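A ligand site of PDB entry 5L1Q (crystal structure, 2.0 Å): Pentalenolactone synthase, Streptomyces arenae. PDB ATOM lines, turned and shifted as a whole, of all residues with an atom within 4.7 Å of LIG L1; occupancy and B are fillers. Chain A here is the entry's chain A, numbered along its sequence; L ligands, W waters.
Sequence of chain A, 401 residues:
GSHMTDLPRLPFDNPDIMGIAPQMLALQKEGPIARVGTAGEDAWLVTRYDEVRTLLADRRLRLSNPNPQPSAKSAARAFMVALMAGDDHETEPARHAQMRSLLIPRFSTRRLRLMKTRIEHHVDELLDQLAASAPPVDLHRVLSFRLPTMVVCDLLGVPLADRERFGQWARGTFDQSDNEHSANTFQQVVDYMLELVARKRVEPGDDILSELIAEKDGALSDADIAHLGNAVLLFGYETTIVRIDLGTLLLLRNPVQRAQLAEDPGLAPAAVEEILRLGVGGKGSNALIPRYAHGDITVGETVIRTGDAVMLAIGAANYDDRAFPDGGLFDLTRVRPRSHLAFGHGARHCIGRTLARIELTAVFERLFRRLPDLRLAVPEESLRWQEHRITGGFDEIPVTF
Residues that only touch LIG L1: Met 84, Phe 107, Leu 155, Phe 235, Gly 236, Thr 239, Thr 240, Arg 243, Leu 276, Ile 289, Ala 342, Phe 343, Gly 344, Ile 351, Gly 352 and Ala 356. Hydrophobic or aromatic side chains within 4 Å of LIG L1: Met 84, His 96, Phe 107, Leu 155, Phe 235, Leu 276, Ile 289, Phe 343 and Ala 356. 21 residues have an atom within 4 Å of LIG L1: Met 84, His 96, Arg 100, Phe 107, Leu 155, Phe 235, Gly 236, Thr 239, Thr 240, Arg 243, Leu 276, Ile 289, Arg 291, Ala 342, Phe 343, Gly 344, Arg 348, Cys 350, Ile 351, Gly 352 and Ala 356. Along chain A the residues within 4 Å of LIG L1 span positions 84 to 356.
N of Cys 350 lies within hydrogen-bond range of O of Phe 343 (3.0 Å). The side-chain sulfur (SG) of Cys 350 sits close to the backbone NH (N) of Gly 352 (3.3 Å). NE2 of His 96 lies close to NH1 of Arg 348. NH1 of Arg 348 sits at hydrogen-bond distance from O of Met 84, at 2.8 Å. The guanidinium group (NE) of Arg 100 sits close to the backbone carbonyl oxygen (O) of Ala 347 (3.3 Å). The guanidinium group (NH1) of Arg 100 sits at hydrogen-bond distance from the backbone carbonyl oxygen (O) of His 349, at 2.8 Å. O of Thr 239 lies within hydrogen-bond range of NH1 of Arg 243 (3.1 Å).
SG of Cys 350 is bound to FE1 of LIG L1, at 2.5 Å. An oxygen (O3) of LIG L1 is in hydrogen-bond range of a ring nitrogen (NE2) of His 96 (2.6 Å). The guanidinium group (NH2) of Arg 291 lies within salt-bridge range of an oxygen (O1) of LIG L1 (2.6 Å). The guanidinium group of Arg 348 lies within salt-bridge range of an oxygen (O4) of LIG L1 (2.8 Å). The guanidinium group of Arg 100 is in salt-bridge range of an oxygen (O3) of LIG L1. The side-chain hydroxyl of Thr 239 lies within hydrogen-bond range of an oxygen (O1) of LG2 L2, at 3.4 Å. NH2 of Arg 243 is in salt-bridge range of O3 of LG2 L2, 2.7 Å away.
Water W3 lies within hydrogen-bond range of O2 of LG2 L2 and O2 of LIG L1. Water W2 lies within hydrogen-bond range of O of Phe 235 and OG1 of Thr 239. Water W4 lies within hydrogen-bond range of O of Phe 235 (2.9 Å), OG1 of Thr 240 (2.9 Å) and N of Thr 239 (3.5 Å).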
ATOM      1  N   LEU A  63     -11.534 -21.768  -8.590  1.00  0.00           N
ATOM      2  CA  LEU A  63     -12.837 -21.590  -7.971  1.00  0.00           C
ATOM      3  C   LEU A  63     -12.711 -21.311  -6.481  1.00  0.00           C
ATOM      4  O   LEU A  63     -13.460 -20.483  -5.938  1.00  0.00           O
ATOM      5  CB  LEU A  63     -13.707 -22.829  -8.213  1.00  0.00           C
ATOM      6  CG  LEU A  63     -15.138 -22.738  -7.659  1.00  0.00           C
ATOM      7  CD1 LEU A  63     -15.987 -21.728  -8.450  1.00  0.00           C
ATOM      8  CD2 LEU A  63     -15.814 -24.123  -7.614  1.00  0.00           C
ATOM      9  N   MET A  84     -18.547 -28.795  -6.492  1.00  0.00           N
ATOM     10  CA  MET A  84     -17.440 -28.678  -7.439  1.00  0.00           C
ATOM     11  C   MET A  84     -16.072 -28.865  -6.789  1.00  0.00           C
ATOM     12  O   MET A  84     -15.058 -28.564  -7.426  1.00  0.00           O
ATOM     13  CB  MET A  84     -17.469 -27.327  -8.167  1.00  0.00           C
ATOM     14  CG  MET A  84     -18.600 -27.221  -9.195  1.00  0.00           C
ATOM     15  SD  MET A  84     -19.071 -25.525  -9.539  1.00  0.00           S
ATOM     16  CE  MET A  84     -17.869 -25.277 -10.876  1.00  0.00           C
ATOM     17  N   HIS A  96     -10.383 -31.899  -6.922  1.00  0.00           N
ATOM     18  CA  HIS A  96     -10.965 -31.584  -8.226  1.00  0.00           C
ATOM     19  C   HIS A  96     -10.427 -32.512  -9.305  1.00  0.00           C
ATOM     20  O   HIS A  96     -11.175 -32.952 -10.175  1.00  0.00           O
ATOM     21  CB  HIS A  96     -10.682 -30.130  -8.621  1.00  0.00           C
ATOM     22  CG  HIS A  96     -11.320 -29.748  -9.922  1.00  0.00           C
ATOM     23  ND1 HIS A  96     -10.590 -29.322 -11.006  1.00  0.00           N
ATOM     24  CD2 HIS A  96     -12.616 -29.774 -10.316  1.00  0.00           C
ATOM     25  CE1 HIS A  96     -11.407 -29.093 -12.019  1.00  0.00           C
ATOM     26  NE2 HIS A  96     -12.647 -29.358 -11.625  1.00  0.00           N
ATOM     27  N   MET A  99     -12.316 -35.702  -9.031  1.00  0.00           N
ATOM     28  CA  MET A  99     -13.677 -35.509  -9.532  1.00  0.00           C
ATOM     29  C   MET A  99     -13.744 -35.668 -11.045  1.00  0.00           C
ATOM     30  O   MET A  99     -14.635 -36.365 -11.573  1.00  0.00           O
ATOM     31  CB  MET A  99     -14.172 -34.130  -9.153  1.00  0.00           C
ATOM     32  CG  MET A  99     -15.467 -33.799  -9.854  1.00  0.00           C
ATOM     33  SD  MET A  99     -16.381 -32.602  -8.904  1.00  0.00           S
ATOM     34  CE  MET A  99     -15.297 -31.213  -9.033  1.00  0.00           C
ATOM     35  N   ARG A 100     -12.867 -34.971 -11.770  1.00  0.00           N
ATOM     36  CA  ARG A 100     -12.917 -35.043 -13.228  1.00  0.00           C
ATOM     37  C   ARG A 100     -12.471 -36.399 -13.737  1.00  0.00           C
ATOM     38  O   ARG A 100     -13.008 -36.897 -14.726  1.00  0.00           O
ATOM     39  CB  ARG A 100     -12.078 -33.909 -13.818  1.00  0.00           C
ATOM     40  CG  ARG A 100     -12.742 -32.567 -13.536  1.00  0.00           C
ATOM     41  CD  ARG A 100     -12.170 -31.456 -14.369  1.00  0.00           C
ATOM     42  NE  ARG A 100     -12.330 -31.639 -15.807  1.00  0.00           N
ATOM     43  CZ  ARG A 100     -13.295 -31.091 -16.545  1.00  0.00           C
ATOM     44  NH1 ARG A 100     -14.229 -30.323 -16.001  1.00  0.00           N
ATOM     45  NH2 ARG A 100     -13.306 -31.298 -17.849  1.00  0.00           N
ATOM     46  N   LEU A 103     -15.579 -38.648 -13.338  1.00  0.00           N
ATOM     47  CA  LEU A 103     -16.784 -38.297 -14.079  1.00  0.00           C
ATOM     48  C   LEU A 103     -16.608 -38.370 -15.599  1.00  0.00           C
ATOM     49  O   LEU A 103     -17.526 -38.820 -16.306  1.00  0.00           O
ATOM     50  CB  LEU A 103     -17.268 -36.892 -13.671  1.00  0.00           C
ATOM     51  CG  LEU A 103     -17.941 -36.760 -12.306  1.00  0.00           C
ATOM     52  CD1 LEU A 103     -18.366 -35.314 -12.003  1.00  0.00           C
ATOM     53  CD2 LEU A 103     -19.131 -37.705 -12.193  1.00  0.00           C
ATOM     54  N   PHE A 107     -19.041 -40.480 -19.469  1.00  0.00           N
ATOM     55  CA  PHE A 107     -19.685 -39.936 -20.649  1.00  0.00           C
ATOM     56  C   PHE A 107     -18.961 -40.477 -21.866  1.00  0.00           C
ATOM     57  O   PHE A 107     -18.483 -39.721 -22.728  1.00  0.00           O
ATOM     58  CB  PHE A 107     -19.698 -38.403 -20.582  1.00  0.00           C
ATOM     59  CG  PHE A 107     -20.489 -37.869 -19.416  1.00  0.00           C
ATOM     60  CD1 PHE A 107     -21.828 -37.502 -19.575  1.00  0.00           C
ATOM     61  CD2 PHE A 107     -19.926 -37.790 -18.145  1.00  0.00           C
ATOM     62  CE1 PHE A 107     -22.574 -37.047 -18.498  1.00  0.00           C
ATOM     63  CE2 PHE A 107     -20.667 -37.345 -17.060  1.00  0.00           C
ATOM     64  CZ  PHE A 107     -22.004 -36.955 -17.241  1.00  0.00           C
ATOM     65  N   LEU A 155     -29.080 -41.487 -16.933  1.00  0.00           N
ATOM     66  CA  LEU A 155     -27.717 -41.492 -16.422  1.00  0.00           C
ATOM     67  C   LEU A 155     -27.640 -42.198 -15.075  1.00  0.00           C
ATOM     68  O   LEU A 155     -26.693 -42.948 -14.812  1.00  0.00           O
ATOM     69  CB  LEU A 155     -27.207 -40.063 -16.269  1.00  0.00           C
ATOM     70  CG  LEU A 155     -26.873 -39.329 -17.553  1.00  0.00           C
ATOM     71  CD1 LEU A 155     -26.416 -37.919 -17.204  1.00  0.00           C
ATOM     72  CD2 LEU A 155     -25.787 -40.104 -18.312  1.00  0.00           C
ATOM     73  N   VAL A 232     -24.002 -34.613 -10.730  1.00  0.00           N
ATOM     74  CA  VAL A 232     -24.684 -34.956 -11.976  1.00  0.00           C
ATOM     75  C   VAL A 232     -26.154 -34.538 -11.915  1.00  0.00           C
ATOM     76  O   VAL A 232     -26.694 -33.963 -12.865  1.00  0.00           O
ATOM     77  CB  VAL A 232     -24.559 -36.468 -12.266  1.00  0.00           C
ATOM     78  CG1 VAL A 232     -25.521 -36.870 -13.401  1.00  0.00           C
ATOM     79  CG2 VAL A 232     -23.135 -36.852 -12.641  1.00  0.00           C
ATOM     80  N   PHE A 235     -26.230 -30.382 -11.582  1.00  0.00           N
ATOM     81  CA  PHE A 235     -25.717 -29.679 -12.752  1.00  0.00           C
ATOM     82  C   PHE A 235     -26.239 -30.250 -14.064  1.00  0.00           C
ATOM     83  O   PHE A 235     -26.081 -29.601 -15.111  1.00  0.00           O
ATOM     84  CB  PHE A 235     -24.177 -29.698 -12.773  1.00  0.00           C
ATOM     85  CG  PHE A 235     -23.526 -29.166 -11.505  1.00  0.00           C
ATOM     86  CD1 PHE A 235     -24.189 -28.267 -10.678  1.00  0.00           C
ATOM     87  CD2 PHE A 235     -22.241 -29.576 -11.155  1.00  0.00           C
ATOM     88  CE1 PHE A 235     -23.598 -27.778  -9.517  1.00  0.00           C
ATOM     89  CE2 PHE A 235     -21.638 -29.109  -9.993  1.00  0.00           C
ATOM     90  CZ  PHE A 235     -22.306 -28.199  -9.174  1.00  0.00           C
ATOM     91  N   GLY A 236     -26.849 -31.432 -14.051  1.00  0.00           N
ATOM     92  CA  GLY A 236     -27.093 -32.154 -15.277  1.00  0.00           C
ATOM     93  C   GLY A 236     -28.429 -31.999 -15.967  1.00  0.00           C
ATOM     94  O   GLY A 236     -28.611 -32.576 -17.040  1.00  0.00           O
ATOM     95  N   THR A 239     -29.665 -26.452 -16.285  1.00  0.00           N
ATOM     96  CA  THR A 239     -29.045 -25.554 -17.266  1.00  0.00           C
ATOM     97  C   THR A 239     -29.467 -25.932 -18.686  1.00  0.00           C
ATOM     98  O   THR A 239     -29.661 -25.045 -19.526  1.00  0.00           O
ATOM     99  CB  THR A 239     -27.515 -25.598 -17.116  1.00  0.00           C
ATOM    100  OG1 THR A 239     -27.163 -25.305 -15.760  1.00  0.00           O
ATOM    101  CG2 THR A 239     -26.859 -24.552 -18.022  1.00  0.00           C
ATOM    102  N   THR A 240     -29.608 -27.235 -18.977  1.00  0.00           N
ATOM    103  CA  THR A 240     -30.084 -27.665 -20.299  1.00  0.00           C
ATOM    104  C   THR A 240     -31.542 -27.232 -20.542  1.00  0.00           C
ATOM    105  O   THR A 240     -31.888 -26.801 -21.650  1.00  0.00           O
ATOM    106  CB  THR A 240     -29.955 -29.177 -20.447  1.00  0.00           C
ATOM    107  OG1 THR A 240     -28.623 -29.562 -20.111  1.00  0.00           O
ATOM    108  CG2 THR A 240     -30.218 -29.617 -21.888  1.00  0.00           C
ATOM    109  N   ARG A 243     -31.538 -23.779 -21.700  1.00  0.00           N
ATOM    110  CA  ARG A 243     -31.072 -23.558 -23.070  1.00  0.00           C
ATOM    111  C   ARG A 243     -32.121 -23.948 -24.109  1.00  0.00           C
ATOM    112  O   ARG A 243     -32.155 -23.355 -25.196  1.00  0.00           O
ATOM    113  CB  ARG A 243     -29.765 -24.309 -23.325  1.00  0.00           C
ATOM    114  CG  ARG A 243     -28.564 -23.790 -22.497  1.00  0.00           C
ATOM    115  CD  ARG A 243     -28.627 -22.279 -22.346  1.00  0.00           C
ATOM    116  NE  ARG A 243     -27.533 -21.709 -21.537  1.00  0.00           N
ATOM    117  CZ  ARG A 243     -27.500 -21.662 -20.206  1.00  0.00           C
ATOM    118  NH1 ARG A 243     -28.496 -22.191 -19.491  1.00  0.00           N
ATOM    119  NH2 ARG A 243     -26.467 -21.096 -19.570  1.00  0.00           N
ATOM    120  N   LEU A 276     -26.257 -21.614 -27.956  1.00  0.00           N
ATOM    121  CA  LEU A 276     -25.410 -21.579 -26.758  1.00  0.00           C
ATOM    122  C   LEU A 276     -24.683 -20.233 -26.644  1.00  0.00           C
ATOM    123  O   LEU A 276     -24.557 -19.676 -25.545  1.00  0.00           O
ATOM    124  CB  LEU A 276     -24.391 -22.714 -26.807  1.00  0.00           C
ATOM    125  CG  LEU A 276     -24.984 -24.122 -26.646  1.00  0.00           C
ATOM    126  CD1 LEU A 276     -24.029 -25.207 -27.130  1.00  0.00           C
ATOM    127  CD2 LEU A 276     -25.433 -24.390 -25.210  1.00  0.00           C
ATOM    128  N   ILE A 289     -18.636 -16.674 -14.771  1.00  0.00           N
ATOM    129  CA  ILE A 289     -17.899 -17.741 -14.097  1.00  0.00           C
ATOM    130  C   ILE A 289     -17.047 -17.089 -13.009  1.00  0.00           C
ATOM    131  O   ILE A 289     -16.183 -16.263 -13.335  1.00  0.00           O
ATOM    132  CB  ILE A 289     -17.034 -18.560 -15.067  1.00  0.00           C
ATOM    133  CG1 ILE A 289     -17.928 -19.355 -16.032  1.00  0.00           C
ATOM    134  CG2 ILE A 289     -16.099 -19.486 -14.290  1.00  0.00           C
ATOM    135  CD1 ILE A 289     -17.148 -20.297 -16.952  1.00  0.00           C
ATOM    136  N   ARG A 291     -14.209 -16.681  -9.965  1.00  0.00           N
ATOM    137  CA  ARG A 291     -12.886 -17.196  -9.618  1.00  0.00           C
ATOM    138  C   ARG A 291     -12.250 -16.305  -8.553  1.00  0.00           C
ATOM    139  O   ARG A 291     -12.695 -15.181  -8.312  1.00  0.00           O
ATOM    140  CB  ARG A 291     -11.959 -17.230 -10.851  1.00  0.00           C
ATOM    141  CG  ARG A 291     -12.383 -18.193 -11.949  1.00  0.00           C
ATOM    142  CD  ARG A 291     -12.234 -19.645 -11.489  1.00  0.00           C
ATOM    143  NE  ARG A 291     -12.489 -20.603 -12.574  1.00  0.00           N
ATOM    144  CZ  ARG A 291     -13.602 -21.306 -12.736  1.00  0.00           C
ATOM    145  NH1 ARG A 291     -14.633 -21.163 -11.893  1.00  0.00           N
ATOM    146  NH2 ARG A 291     -13.699 -22.160 -13.754  1.00  0.00           N
ATOM    147  N   ILE A 314     -18.599 -14.924 -19.509  1.00  0.00           N
ATOM    148  CA  ILE A 314     -18.646 -15.741 -20.711  1.00  0.00           C
ATOM    149  C   ILE A 314     -19.759 -15.289 -21.643  1.00  0.00           C
ATOM    150  O   ILE A 314     -19.637 -15.394 -22.867  1.00  0.00           O
ATOM    151  CB  ILE A 314     -18.796 -17.245 -20.338  1.00  0.00           C
ATOM    152  CG1 ILE A 314     -20.012 -17.475 -19.442  1.00  0.00           C
ATOM    153  CG2 ILE A 314     -17.489 -17.764 -19.709  1.00  0.00           C
ATOM    154  CD1 ILE A 314     -20.262 -18.954 -19.053  1.00  0.00           C
ATOM    155  N   ALA A 342     -19.781 -20.856 -23.700  1.00  0.00           N
ATOM    156  CA  ALA A 342     -20.962 -21.160 -22.877  1.00  0.00           C
ATOM    157  C   ALA A 342     -20.748 -22.362 -21.963  1.00  0.00           C
ATOM    158  O   ALA A 342     -21.421 -22.471 -20.944  1.00  0.00           O
ATOM    159  CB  ALA A 342     -22.194 -21.404 -23.751  1.00  0.00           C
ATOM    160  N   PHE A 343     -19.853 -23.283 -22.335  1.00  0.00           N
ATOM    161  CA  PHE A 343     -19.485 -24.404 -21.474  1.00  0.00           C
ATOM    162  C   PHE A 343     -18.229 -24.141 -20.657  1.00  0.00           C
ATOM    163  O   PHE A 343     -17.697 -25.061 -20.008  1.00  0.00           O
ATOM    164  CB  PHE A 343     -19.267 -25.669 -22.306  1.00  0.00           C
ATOM    165  CG  PHE A 343     -20.508 -26.205 -22.958  1.00  0.00           C
ATOM    166  CD1 PHE A 343     -21.583 -26.663 -22.191  1.00  0.00           C
ATOM    167  CD2 PHE A 343     -20.594 -26.298 -24.353  1.00  0.00           C
ATOM    168  CE1 PHE A 343     -22.737 -27.177 -22.812  1.00  0.00           C
ATOM    169  CE2 PHE A 343     -21.735 -26.811 -24.981  1.00  0.00           C
ATOM    170  CZ  PHE A 343     -22.807 -27.239 -24.215  1.00  0.00           C
ATOM    171  N   GLY A 344     -17.725 -22.924 -20.675  1.00  0.00           N
ATOM    172  CA  GLY A 344     -16.458 -22.676 -20.020  1.00  0.00           C
ATOM    173  C   GLY A 344     -15.279 -23.112 -20.877  1.00  0.00           C
ATOM    174  O   GLY A 344     -15.377 -23.259 -22.101  1.00  0.00           O
ATOM    175  N   ALA A 347      -9.602 -25.855 -16.927  1.00  0.00           N
ATOM    176  CA  ALA A 347      -9.640 -26.926 -15.920  1.00  0.00           C
ATOM    177  C   ALA A 347     -11.057 -27.404 -15.625  1.00  0.00           C
ATOM    178  O   ALA A 347     -11.251 -28.596 -15.341  1.00  0.00           O
ATOM    179  CB  ALA A 347      -8.973 -26.449 -14.621  1.00  0.00           C
ATOM    180  N   ARG A 348     -12.052 -26.526 -15.673  1.00  0.00           N
ATOM    181  CA  ARG A 348     -13.411 -26.921 -15.279  1.00  0.00           C
ATOM    182  C   ARG A 348     -14.391 -26.953 -16.454  1.00  0.00           C
ATOM    183  O   ARG A 348     -15.600 -26.943 -16.244  1.00  0.00           O
ATOM    184  CB  ARG A 348     -13.917 -25.992 -14.172  1.00  0.00           C
ATOM    185  CG  ARG A 348     -13.079 -26.101 -12.878  1.00  0.00           C
ATOM    186  CD  ARG A 348     -13.649 -25.275 -11.734  1.00  0.00           C
ATOM    187  NE  ARG A 348     -13.021 -25.566 -10.442  1.00  0.00           N
ATOM    188  CZ  ARG A 348     -13.472 -26.468  -9.568  1.00  0.00           C
ATOM    189  NH1 ARG A 348     -14.550 -27.181  -9.862  1.00  0.00           N
ATOM    190  NH2 ARG A 348     -12.838 -26.669  -8.406  1.00  0.00           N
ATOM    191  N   HIS A 349     -13.870 -27.041 -17.685  1.00  0.00           N
ATOM    192  CA  HIS A 349     -14.681 -27.187 -18.893  1.00  0.00           C
ATOM    193  C   HIS A 349     -15.773 -28.241 -18.689  1.00  0.00           C
ATOM    194  O   HIS A 349     -15.496 -29.371 -18.312  1.00  0.00           O
ATOM    195  CB  HIS A 349     -13.765 -27.577 -20.058  1.00  0.00           C
ATOM    196  CG  HIS A 349     -14.317 -27.253 -21.412  1.00  0.00           C
ATOM    197  ND1 HIS A 349     -13.654 -27.590 -22.567  1.00  0.00           N
ATOM    198  CD2 HIS A 349     -15.457 -26.639 -21.797  1.00  0.00           C
ATOM    199  CE1 HIS A 349     -14.356 -27.198 -23.609  1.00  0.00           C
ATOM    200  NE2 HIS A 349     -15.460 -26.607 -23.172  1.00  0.00           N
ATOM    201  N   CYS A 350     -17.009 -27.839 -18.980  1.00  0.00           N
ATOM    202  CA  CYS A 350     -18.211 -28.602 -18.633  1.00  0.00           C
ATOM    203  C   CYS A 350     -18.082 -30.070 -19.023  1.00  0.00           C
ATOM    204  O   CYS A 350     -17.862 -30.403 -20.187  1.00  0.00           O
ATOM    205  CB  CYS A 350     -19.417 -27.976 -19.361  1.00  0.00           C
ATOM    206  SG  CYS A 350     -20.895 -29.049 -19.397  1.00  0.00           S
ATOM    207  N   ILE A 351     -18.250 -30.951 -18.026  1.00  0.00           N
ATOM    208  CA  ILE A 351     -18.089 -32.386 -18.289  1.00  0.00           C
ATOM    209  C   ILE A 351     -19.231 -32.926 -19.164  1.00  0.00           C
ATOM    210  O   ILE A 351     -19.029 -33.851 -19.950  1.00  0.00           O
ATOM    211  CB  ILE A 351     -17.976 -33.157 -16.952  1.00  0.00           C
ATOM    212  CG1 ILE A 351     -16.596 -32.933 -16.321  1.00  0.00           C
ATOM    213  CG2 ILE A 351     -18.222 -34.668 -17.164  1.00  0.00           C
ATOM    214  CD1 ILE A 351     -16.479 -33.484 -14.934  1.00  0.00           C
ATOM    215  N   GLY A 352     -20.422 -32.344 -19.069  1.00  0.00           N
ATOM    216  CA  GLY A 352     -21.566 -32.850 -19.818  1.00  0.00           C
ATOM    217  C   GLY A 352     -21.779 -32.266 -21.195  1.00  0.00           C
ATOM    218  O   GLY A 352     -22.815 -32.540 -21.820  1.00  0.00           O
ATOM    219  N   LEU A 355     -23.013 -34.383 -24.186  1.00  0.00           N
ATOM    220  CA  LEU A 355     -24.388 -34.828 -23.968  1.00  0.00           C
ATOM    221  C   LEU A 355     -25.378 -33.679 -24.145  1.00  0.00           C
ATOM    222  O   LEU A 355     -26.453 -33.846 -24.738  1.00  0.00           O
ATOM    223  CB  LEU A 355     -24.489 -35.438 -22.566  1.00  0.00           C
ATOM    224  CG  LEU A 355     -25.863 -35.998 -22.139  1.00  0.00           C
ATOM    225  CD1 LEU A 355     -26.352 -37.039 -23.153  1.00  0.00           C
ATOM    226  CD2 LEU A 355     -25.802 -36.593 -20.732  1.00  0.00           C
ATOM    227  N   ALA A 356     -25.058 -32.506 -23.587  1.00  0.00           N
ATOM    228  CA  ALA A 356     -25.954 -31.363 -23.711  1.00  0.00           C
ATOM    229  C   ALA A 356     -26.154 -30.992 -25.181  1.00  0.00           C
ATOM    230  O   ALA A 356     -27.276 -30.686 -25.599  1.00  0.00           O
ATOM    231  CB  ALA A 356     -25.401 -30.167 -22.912  1.00  0.00           C
ATOM    232  N   GLU A 359     -28.594 -33.448 -26.761  1.00  0.00           N
ATOM    233  CA  GLU A 359     -29.988 -33.142 -26.411  1.00  0.00           C
ATOM    234  C   GLU A 359     -30.508 -31.962 -27.222  1.00  0.00           C
ATOM    235  O   GLU A 359     -31.608 -32.039 -27.791  1.00  0.00           O
ATOM    236  CB  GLU A 359     -30.091 -32.807 -24.924  1.00  0.00           C
ATOM    237  CG  GLU A 359     -29.816 -33.952 -24.002  1.00  0.00           C
ATOM    238  CD  GLU A 359     -30.055 -33.582 -22.549  1.00  0.00           C
ATOM    239  OE1 GLU A 359     -29.146 -33.779 -21.731  1.00  0.00           O
ATOM    240  OE2 GLU A 359     -31.165 -33.085 -22.236  1.00  0.00           O
ATOM    241  N   LEU A 360     -29.767 -30.853 -27.235  1.00  0.00           N
ATOM    242  CA  LEU A 360     -30.218 -29.658 -27.932  1.00  0.00           C
ATOM    243  C   LEU A 360     -30.335 -29.894 -29.437  1.00  0.00           C
ATOM    244  O   LEU A 360     -31.277 -29.427 -30.080  1.00  0.00           O
ATOM    245  CB  LEU A 360     -29.255 -28.496 -27.655  1.00  0.00           C
ATOM    246  CG  LEU A 360     -29.191 -27.896 -26.241  1.00  0.00           C
ATOM    247  CD1 LEU A 360     -28.087 -26.828 -26.133  1.00  0.00           C
ATOM    248  CD2 LEU A 360     -30.549 -27.323 -25.798  1.00  0.00           C
HETATM  249  C1  LIG L   1     -19.339 -27.290 -15.429  1.00  0.00           C
HETATM  250  C2  LIG L   1     -22.307 -25.047 -18.563  1.00  0.00           C
HETATM  251  C3  LIG L   1     -24.931 -29.068 -19.028  1.00  0.00           C
HETATM  252  C4  LIG L   1     -22.081 -31.315 -15.812  1.00  0.00           C
HETATM  253  C5  LIG L   1     -19.870 -26.341 -16.262  1.00  0.00           C
HETATM  254  C6  LIG L   1     -19.332 -25.009 -16.502  1.00  0.00           C
HETATM  255  C7  LIG L   1     -20.161 -24.403 -17.378  1.00  0.00           C
HETATM  256  C8  LIG L   1     -21.246 -25.317 -17.709  1.00  0.00           C
HETATM  257  C9  LIG L   1     -20.042 -22.957 -17.927  1.00  0.00           C
HETATM  258  C10 LIG L   1     -18.020 -24.422 -15.884  1.00  0.00           C
HETATM  259  C11 LIG L   1     -18.230 -23.705 -14.539  1.00  0.00           C
HETATM  260  C12 LIG L   1     -16.941 -23.108 -14.036  1.00  0.00           C
HETATM  261  O1  LIG L   1     -15.909 -23.124 -14.769  1.00  0.00           O
HETATM  262  O2  LIG L   1     -16.932 -22.579 -12.876  1.00  0.00           O
HETATM  263  C13 LIG L   1     -23.282 -25.906 -18.991  1.00  0.00           C
HETATM  264  C14 LIG L   1     -24.329 -25.667 -19.978  1.00  0.00           C
HETATM  265  C15 LIG L   1     -25.052 -26.795 -20.070  1.00  0.00           C
HETATM  266  C16 LIG L   1     -24.472 -27.775 -19.184  1.00  0.00           C
HETATM  267  C17 LIG L   1     -24.568 -24.341 -20.755  1.00  0.00           C
HETATM  268  C18 LIG L   1     -26.273 -27.155 -20.953  1.00  0.00           C
HETATM  269  C19 LIG L   1     -26.536 -26.584 -22.141  1.00  0.00           C
HETATM  270  C20 LIG L   1     -24.359 -30.053 -18.262  1.00  0.00           C
HETATM  271  C21 LIG L   1     -24.747 -31.446 -18.270  1.00  0.00           C
HETATM  272  C22 LIG L   1     -23.964 -32.076 -17.380  1.00  0.00           C
HETATM  273  C23 LIG L   1     -23.063 -31.100 -16.775  1.00  0.00           C
HETATM  274  C24 LIG L   1     -25.878 -32.014 -19.194  1.00  0.00           C
HETATM  275  C25 LIG L   1     -23.961 -33.583 -16.981  1.00  0.00           C
HETATM  276  C26 LIG L   1     -25.005 -34.422 -17.171  1.00  0.00           C
HETATM  277  C27 LIG L   1     -21.126 -30.407 -15.394  1.00  0.00           C
HETATM  278  C28 LIG L   1     -20.166 -30.610 -14.333  1.00  0.00           C
HETATM  279  C29 LIG L   1     -19.412 -29.505 -14.204  1.00  0.00           C
HETATM  280  C30 LIG L   1     -19.873 -28.545 -15.191  1.00  0.00           C
HETATM  281  C31 LIG L   1     -20.074 -31.912 -13.505  1.00  0.00           C
HETATM  282  C32 LIG L   1     -18.259 -29.253 -13.221  1.00  0.00           C
HETATM  283  C33 LIG L   1     -16.906 -29.386 -13.946  1.00  0.00           C
HETATM  284  C34 LIG L   1     -15.769 -28.946 -13.047  1.00  0.00           C
HETATM  285  O3  LIG L   1     -14.633 -29.448 -13.266  1.00  0.00           O
HETATM  286  O4  LIG L   1     -15.987 -28.128 -12.110  1.00  0.00           O
HETATM  287  N1  LIG L   1     -21.030 -26.492 -17.008  1.00  0.00           N
HETATM  288  N2  LIG L   1     -23.412 -27.198 -18.525  1.00  0.00           N
HETATM  289  N3  LIG L   1     -23.338 -29.871 -17.331  1.00  0.00           N
HETATM  290  N4  LIG L   1     -20.917 -29.138 -15.884  1.00  0.00           N
HETATM  291 FE1  LIG L   1     -22.080 -28.227 -17.356  1.00  0.00          FE
HETATM  292  C1  LG2 L   2     -22.195 -24.620 -14.501  1.00  0.00           C
HETATM  293  C2  LG2 L   2     -22.751 -24.764 -13.066  1.00  0.00           C
HETATM  294  C3  LG2 L   2     -22.489 -23.343 -12.490  1.00  0.00           C
HETATM  295  C4  LG2 L   2     -22.780 -22.350 -13.677  1.00  0.00           C
HETATM  296  C5  LG2 L   2     -24.251 -21.863 -13.810  1.00  0.00           C
HETATM  297  C6  LG2 L   2     -24.398 -21.754 -15.340  1.00  0.00           C
HETATM  298  C7  LG2 L   2     -21.845 -21.120 -13.510  1.00  0.00           C
HETATM  299  C8  LG2 L   2     -21.294 -20.365 -14.702  1.00  0.00           C
HETATM  300  C9  LG2 L   2     -22.170 -20.428 -12.325  1.00  0.00           C
HETATM  301  C10 LG2 L   2     -21.904 -25.805 -12.318  1.00  0.00           C
HETATM  302  C11 LG2 L   2     -24.225 -25.201 -13.001  1.00  0.00           C
HETATM  303  C12 LG2 L   2     -24.444 -20.456 -13.193  1.00  0.00           C
HETATM  304  C13 LG2 L   2     -23.903 -23.134 -15.734  1.00  0.00           C
HETATM  305  C14 LG2 L   2     -25.825 -21.513 -15.846  1.00  0.00           C
HETATM  306  C15 LG2 L   2     -22.549 -23.179 -14.982  1.00  0.00           C
HETATM  307  O1  LG2 L   2     -26.769 -21.989 -15.186  1.00  0.00           O
HETATM  308  O2  LG2 L   2     -21.299 -20.174 -11.487  1.00  0.00           O
HETATM  309  O3  LG2 L   2     -25.962 -20.878 -16.917  1.00  0.00           O
HETATM  310  O4  LG2 L   2     -23.508 -20.159 -12.106  1.00  0.00           O
HETATM  311  O5  LG2 L   2     -20.458 -21.211 -13.846  1.00  0.00           O
HETATM  312  O   HOH W   1     -14.740 -23.566 -17.233  1.00  0.00           O
HETATM  313  O   HOH W   2     -24.558 -27.275 -15.783  1.00  0.00           O
HETATM  314  O   HOH W   3     -19.030 -21.710 -11.237  1.00  0.00           O
HETATM  315  O   HOH W   4     -27.779 -29.186 -17.373  1.00  0.00           O
